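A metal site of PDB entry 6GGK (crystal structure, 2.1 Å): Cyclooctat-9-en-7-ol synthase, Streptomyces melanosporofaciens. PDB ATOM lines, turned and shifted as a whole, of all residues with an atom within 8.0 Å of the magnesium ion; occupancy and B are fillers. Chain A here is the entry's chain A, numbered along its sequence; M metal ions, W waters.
The magnesium ion is bound by water W3 (2.1 Å), the side-chain carboxylate of Glu 228 (2.2 Å), water W1 (2.2 Å), water W2 (2.3 Å), the side-chain amide oxygen of Asn 220 (2.3 Å) and the side-chain hydroxyl of Ser 224 (2.4 Å). The magnesium ion has six donor atoms within binding distance.
Water W1 lies within hydrogen-bond range of the side-chain carboxylate of Asp 221 (2.7 Å), the side-chain carboxylate of Glu 228 (2.8 Å) and the guanidinium group of Arg 177 (3.1 Å).
Of the 19 residues printed, 3 come within 4 Å of the magnesium ion. The nearest printed residue that does not touch the magnesium ion is Arg 177 (4.3 Å).
OE2 of Glu 228 sits at hydrogen-bond distance from ND2 of Asn 236, at 3.0 Å. The backbone carbonyl oxygen (O) of Glu 228 lies within hydrogen-bond range of the backbone NH (N) of Gln 233, 3.0 Å away.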
ATOM      1  N   ASP A 110      18.137  -0.229 -20.931  1.00  0.00           N
ATOM      2  CA  ASP A 110      18.680  -1.269 -21.805  1.00  0.00           C
ATOM      3  C   ASP A 110      18.160  -1.122 -23.229  1.00  0.00           C
ATOM      4  O   ASP A 110      18.827  -1.548 -24.175  1.00  0.00           O
ATOM      5  CB  ASP A 110      18.342  -2.637 -21.203  1.00  0.00           C
ATOM      6  CG  ASP A 110      18.927  -3.785 -21.982  1.00  0.00           C
ATOM      7  OD1 ASP A 110      18.285  -4.205 -22.981  1.00  0.00           O
ATOM      8  OD2 ASP A 110      20.005  -4.282 -21.603  1.00  0.00           O
ATOM      9  N   TYR A 173      27.695 -19.289 -22.716  1.00  0.00           N
ATOM     10  CA  TYR A 173      26.672 -18.268 -22.946  1.00  0.00           C
ATOM     11  C   TYR A 173      25.783 -18.093 -21.710  1.00  0.00           C
ATOM     12  O   TYR A 173      25.564 -16.958 -21.254  1.00  0.00           O
ATOM     13  CB  TYR A 173      25.836 -18.644 -24.166  1.00  0.00           C
ATOM     14  CG  TYR A 173      24.575 -17.816 -24.283  1.00  0.00           C
ATOM     15  CD1 TYR A 173      24.627 -16.499 -24.728  1.00  0.00           C
ATOM     16  CD2 TYR A 173      23.338 -18.336 -23.932  1.00  0.00           C
ATOM     17  CE1 TYR A 173      23.479 -15.738 -24.841  1.00  0.00           C
ATOM     18  CE2 TYR A 173      22.180 -17.574 -24.046  1.00  0.00           C
ATOM     19  CZ  TYR A 173      22.260 -16.276 -24.499  1.00  0.00           C
ATOM     20  OH  TYR A 173      21.130 -15.524 -24.600  1.00  0.00           O
ATOM     21  N   ARG A 177      24.998 -15.083 -19.091  1.00  0.00           N
ATOM     22  CA  ARG A 177      23.646 -14.545 -19.002  1.00  0.00           C
ATOM     23  C   ARG A 177      23.137 -14.431 -17.573  1.00  0.00           C
ATOM     24  O   ARG A 177      22.247 -13.596 -17.322  1.00  0.00           O
ATOM     25  CB  ARG A 177      22.694 -15.407 -19.836  1.00  0.00           C
ATOM     26  CG  ARG A 177      22.836 -15.109 -21.308  1.00  0.00           C
ATOM     27  CD  ARG A 177      22.355 -13.682 -21.657  1.00  0.00           C
ATOM     28  NE  ARG A 177      21.143 -13.731 -22.489  1.00  0.00           N
ATOM     29  CZ  ARG A 177      20.330 -12.701 -22.684  1.00  0.00           C
ATOM     30  NH1 ARG A 177      20.589 -11.531 -22.117  1.00  0.00           N
ATOM     31  NH2 ARG A 177      19.249 -12.840 -23.448  1.00  0.00           N
ATOM     32  N   ASP A 180      23.914 -10.939 -17.501  1.00  0.00           N
ATOM     33  CA  ASP A 180      23.500 -10.081 -18.611  1.00  0.00           C
ATOM     34  C   ASP A 180      21.989 -10.093 -18.818  1.00  0.00           C
ATOM     35  O   ASP A 180      21.440  -9.098 -19.289  1.00  0.00           O
ATOM     36  CB  ASP A 180      24.211 -10.502 -19.898  1.00  0.00           C
ATOM     37  CG  ASP A 180      23.765  -9.671 -21.088  1.00  0.00           C
ATOM     38  OD1 ASP A 180      24.254  -8.538 -21.227  1.00  0.00           O
ATOM     39  OD2 ASP A 180      22.919 -10.146 -21.874  1.00  0.00           O
ATOM     40  N   ILE A 181      21.299 -11.181 -18.468  1.00  0.00           N
ATOM     41  CA  ILE A 181      19.847 -11.126 -18.599  1.00  0.00           C
ATOM     42  C   ILE A 181      19.207 -10.480 -17.380  1.00  0.00           C
ATOM     43  O   ILE A 181      17.990 -10.247 -17.369  1.00  0.00           O
ATOM     44  CB  ILE A 181      19.254 -12.521 -18.859  1.00  0.00           C
ATOM     45  CG1 ILE A 181      17.851 -12.391 -19.493  1.00  0.00           C
ATOM     46  CG2 ILE A 181      19.152 -13.307 -17.587  1.00  0.00           C
ATOM     47  CD1 ILE A 181      17.565 -13.327 -20.592  1.00  0.00           C
ATOM     48  N   LEU A 216      14.745 -18.858 -17.744  1.00  0.00           N
ATOM     49  CA  LEU A 216      14.421 -17.485 -18.156  1.00  0.00           C
ATOM     50  C   LEU A 216      15.039 -17.160 -19.523  1.00  0.00           C
ATOM     51  O   LEU A 216      14.377 -16.577 -20.393  1.00  0.00           O
ATOM     52  CB  LEU A 216      14.917 -16.489 -17.110  1.00  0.00           C
ATOM     53  CG  LEU A 216      14.175 -16.491 -15.789  1.00  0.00           C
ATOM     54  CD1 LEU A 216      14.981 -15.700 -14.740  1.00  0.00           C
ATOM     55  CD2 LEU A 216      12.784 -15.900 -15.988  1.00  0.00           C
ATOM     56  N   THR A 217      16.302 -17.512 -19.727  1.00  0.00           N
ATOM     57  CA  THR A 217      17.000 -17.091 -20.939  1.00  0.00           C
ATOM     58  C   THR A 217      16.512 -17.862 -22.171  1.00  0.00           C
ATOM     59  O   THR A 217      16.354 -17.269 -23.247  1.00  0.00           O
ATOM     60  CB  THR A 217      18.502 -17.263 -20.768  1.00  0.00           C
ATOM     61  OG1 THR A 217      18.912 -16.587 -19.575  1.00  0.00           O
ATOM     62  CG2 THR A 217      19.251 -16.691 -21.983  1.00  0.00           C
ATOM     63  N   VAL A 219      13.538 -19.147 -22.836  1.00  0.00           N
ATOM     64  CA  VAL A 219      12.246 -18.576 -23.228  1.00  0.00           C
ATOM     65  C   VAL A 219      12.435 -17.194 -23.845  1.00  0.00           C
ATOM     66  O   VAL A 219      11.963 -16.917 -24.944  1.00  0.00           O
ATOM     67  CB  VAL A 219      11.297 -18.520 -22.032  1.00  0.00           C
ATOM     68  CG1 VAL A 219      10.192 -17.469 -22.300  1.00  0.00           C
ATOM     69  CG2 VAL A 219      10.713 -19.885 -21.747  1.00  0.00           C
ATOM     70  N   ASN A 220      13.124 -16.293 -23.126  1.00  0.00           N
ATOM     71  CA  ASN A 220      13.342 -14.945 -23.632  1.00  0.00           C
ATOM     72  C   ASN A 220      14.054 -14.970 -24.982  1.00  0.00           C
ATOM     73  O   ASN A 220      13.708 -14.203 -25.887  1.00  0.00           O
ATOM     74  CB  ASN A 220      14.119 -14.142 -22.582  1.00  0.00           C
ATOM     75  CG  ASN A 220      14.575 -12.764 -23.082  1.00  0.00           C
ATOM     76  OD1 ASN A 220      15.361 -12.651 -24.016  1.00  0.00           O
ATOM     77  ND2 ASN A 220      14.125 -11.723 -22.412  1.00  0.00           N
ATOM     78  N   ASP A 221      15.043 -15.850 -25.126  1.00  0.00           N
ATOM     79  CA  ASP A 221      15.799 -15.890 -26.373  1.00  0.00           C
ATOM     80  C   ASP A 221      14.935 -16.341 -27.541  1.00  0.00           C
ATOM     81  O   ASP A 221      15.019 -15.772 -28.623  1.00  0.00           O
ATOM     82  CB  ASP A 221      17.015 -16.811 -26.247  1.00  0.00           C
ATOM     83  CG  ASP A 221      18.173 -16.171 -25.487  1.00  0.00           C
ATOM     84  OD1 ASP A 221      18.086 -14.988 -25.114  1.00  0.00           O
ATOM     85  OD2 ASP A 221      19.191 -16.861 -25.266  1.00  0.00           O
ATOM     86  N   PHE A 222      14.114 -17.373 -27.349  1.00  0.00           N
ATOM     87  CA  PHE A 222      13.289 -17.844 -28.458  1.00  0.00           C
ATOM     88  C   PHE A 222      12.363 -16.739 -28.970  1.00  0.00           C
ATOM     89  O   PHE A 222      12.272 -16.492 -30.184  1.00  0.00           O
ATOM     90  CB  PHE A 222      12.482 -19.066 -28.060  1.00  0.00           C
ATOM     91  CG  PHE A 222      11.679 -19.615 -29.183  1.00  0.00           C
ATOM     92  CD1 PHE A 222      12.301 -20.311 -30.201  1.00  0.00           C
ATOM     93  CD2 PHE A 222      10.309 -19.390 -29.242  1.00  0.00           C
ATOM     94  CE1 PHE A 222      11.587 -20.799 -31.257  1.00  0.00           C
ATOM     95  CE2 PHE A 222       9.576 -19.876 -30.301  1.00  0.00           C
ATOM     96  CZ  PHE A 222      10.217 -20.582 -31.322  1.00  0.00           C
ATOM     97  N   TYR A 223      11.666 -16.046 -28.062  1.00  0.00           N
ATOM     98  CA  TYR A 223      10.683 -15.085 -28.530  1.00  0.00           C
ATOM     99  C   TYR A 223      11.298 -13.743 -28.902  1.00  0.00           C
ATOM    100  O   TYR A 223      10.588 -12.892 -29.444  1.00  0.00           O
ATOM    101  CB  TYR A 223       9.573 -14.896 -27.493  1.00  0.00           C
ATOM    102  CG  TYR A 223       8.765 -16.155 -27.313  1.00  0.00           C
ATOM    103  CD1 TYR A 223       7.802 -16.530 -28.247  1.00  0.00           C
ATOM    104  CD2 TYR A 223       9.001 -16.996 -26.224  1.00  0.00           C
ATOM    105  CE1 TYR A 223       7.081 -17.706 -28.098  1.00  0.00           C
ATOM    106  CE2 TYR A 223       8.298 -18.188 -26.069  1.00  0.00           C
ATOM    107  CZ  TYR A 223       7.319 -18.533 -27.010  1.00  0.00           C
ATOM    108  OH  TYR A 223       6.607 -19.699 -26.839  1.00  0.00           O
ATOM    109  N   SER A 224      12.593 -13.525 -28.648  1.00  0.00           N
ATOM    110  CA  SER A 224      13.224 -12.288 -29.080  1.00  0.00           C
ATOM    111  C   SER A 224      14.321 -12.512 -30.121  1.00  0.00           C
ATOM    112  O   SER A 224      15.025 -11.557 -30.477  1.00  0.00           O
ATOM    113  CB  SER A 224      13.769 -11.500 -27.871  1.00  0.00           C
ATOM    114  OG  SER A 224      14.834 -12.153 -27.216  1.00  0.00           O
ATOM    115  N   TYR A 225      14.430 -13.736 -30.672  1.00  0.00           N
ATOM    116  CA  TYR A 225      15.459 -14.030 -31.668  1.00  0.00           C
ATOM    117  C   TYR A 225      15.304 -13.158 -32.918  1.00  0.00           C
ATOM    118  O   TYR A 225      16.267 -12.499 -33.350  1.00  0.00           O
ATOM    119  CB  TYR A 225      15.417 -15.505 -32.049  1.00  0.00           C
ATOM    120  CG  TYR A 225      16.426 -15.925 -33.093  1.00  0.00           C
ATOM    121  CD1 TYR A 225      16.131 -15.846 -34.447  1.00  0.00           C
ATOM    122  CD2 TYR A 225      17.672 -16.413 -32.728  1.00  0.00           C
ATOM    123  CE1 TYR A 225      17.041 -16.234 -35.416  1.00  0.00           C
ATOM    124  CE2 TYR A 225      18.601 -16.811 -33.700  1.00  0.00           C
ATOM    125  CZ  TYR A 225      18.277 -16.713 -35.046  1.00  0.00           C
ATOM    126  OH  TYR A 225      19.189 -17.094 -36.023  1.00  0.00           O
ATOM    127  N   ARG A 227      13.902 -10.355 -33.588  1.00  0.00           N
ATOM    128  CA  ARG A 227      14.179  -8.941 -33.382  1.00  0.00           C
ATOM    129  C   ARG A 227      15.665  -8.698 -33.149  1.00  0.00           C
ATOM    130  O   ARG A 227      16.257  -7.777 -33.725  1.00  0.00           O
ATOM    131  CB  ARG A 227      13.365  -8.424 -32.203  1.00  0.00           C
ATOM    132  CG  ARG A 227      13.488  -6.935 -31.994  1.00  0.00           C
ATOM    133  CD  ARG A 227      12.975  -6.532 -30.619  1.00  0.00           C
ATOM    134  NE  ARG A 227      14.024  -5.860 -29.849  1.00  0.00           N
ATOM    135  CZ  ARG A 227      14.379  -4.592 -29.999  1.00  0.00           C
ATOM    136  NH1 ARG A 227      13.777  -3.830 -30.910  1.00  0.00           N
ATOM    137  NH2 ARG A 227      15.349  -4.069 -29.246  1.00  0.00           N
ATOM    138  N   GLU A 228      16.291  -9.534 -32.324  1.00  0.00           N
ATOM    139  CA  GLU A 228      17.676  -9.278 -31.956  1.00  0.00           C
ATOM    140  C   GLU A 228      18.617  -9.525 -33.131  1.00  0.00           C
ATOM    141  O   GLU A 228      19.511  -8.708 -33.388  1.00  0.00           O
ATOM    142  CB  GLU A 228      18.053 -10.131 -30.737  1.00  0.00           C
ATOM    143  CG  GLU A 228      17.279  -9.683 -29.484  1.00  0.00           C
ATOM    144  CD  GLU A 228      17.485 -10.595 -28.264  1.00  0.00           C
ATOM    145  OE1 GLU A 228      17.051 -10.219 -27.155  1.00  0.00           O
ATOM    146  OE2 GLU A 228      18.081 -11.683 -28.422  1.00  0.00           O
ATOM    147  N   GLN A 233      22.403  -8.194 -32.909  1.00  0.00           N
ATOM    148  CA  GLN A 233      22.823  -8.583 -31.576  1.00  0.00           C
ATOM    149  C   GLN A 233      23.126 -10.079 -31.515  1.00  0.00           C
ATOM    150  O   GLN A 233      22.496 -10.883 -32.199  1.00  0.00           O
ATOM    151  CB  GLN A 233      21.766  -8.221 -30.536  1.00  0.00           C
ATOM    152  CG  GLN A 233      21.528  -6.748 -30.382  1.00  0.00           C
ATOM    153  CD  GLN A 233      20.267  -6.455 -29.598  1.00  0.00           C
ATOM    154  OE1 GLN A 233      19.940  -7.155 -28.638  1.00  0.00           O
ATOM    155  NE2 GLN A 233      19.552  -5.420 -30.019  1.00  0.00           N
ATOM    156  N   THR A 235      23.589 -11.783 -28.337  1.00  0.00           N
ATOM    157  CA  THR A 235      23.285 -12.353 -27.032  1.00  0.00           C
ATOM    158  C   THR A 235      21.979 -13.146 -27.118  1.00  0.00           C
ATOM    159  O   THR A 235      20.924 -12.736 -26.628  1.00  0.00           O
ATOM    160  CB  THR A 235      23.237 -11.269 -25.960  1.00  0.00           C
ATOM    161  OG1 THR A 235      24.472 -10.531 -25.984  1.00  0.00           O
ATOM    162  CG2 THR A 235      23.102 -11.878 -24.589  1.00  0.00           C
ATOM    163  N   ASN A 236      22.062 -14.308 -27.769  1.00  0.00           N
ATOM    164  CA  ASN A 236      20.882 -15.159 -27.929  1.00  0.00           C
ATOM    165  C   ASN A 236      21.346 -16.571 -28.235  1.00  0.00           C
ATOM    166  O   ASN A 236      22.094 -16.788 -29.196  1.00  0.00           O
ATOM    167  CB  ASN A 236      19.987 -14.640 -29.059  1.00  0.00           C
ATOM    168  CG  ASN A 236      18.666 -15.362 -29.122  1.00  0.00           C
ATOM    169  OD1 ASN A 236      18.621 -16.560 -29.387  1.00  0.00           O
ATOM    170  ND2 ASN A 236      17.588 -14.635 -28.872  1.00  0.00           N
HETATM  171 MG    MG M   1      15.940 -10.944 -25.461  1.00  0.00          MG
HETATM  172  O   HOH W   1      17.371 -12.521 -25.882  1.00  0.00           O
HETATM  173  O   HOH W   2      17.615 -10.262 -24.065  1.00  0.00           O
HETATM  174  O   HOH W   3      14.367  -9.717 -24.955  1.00  0.00           O
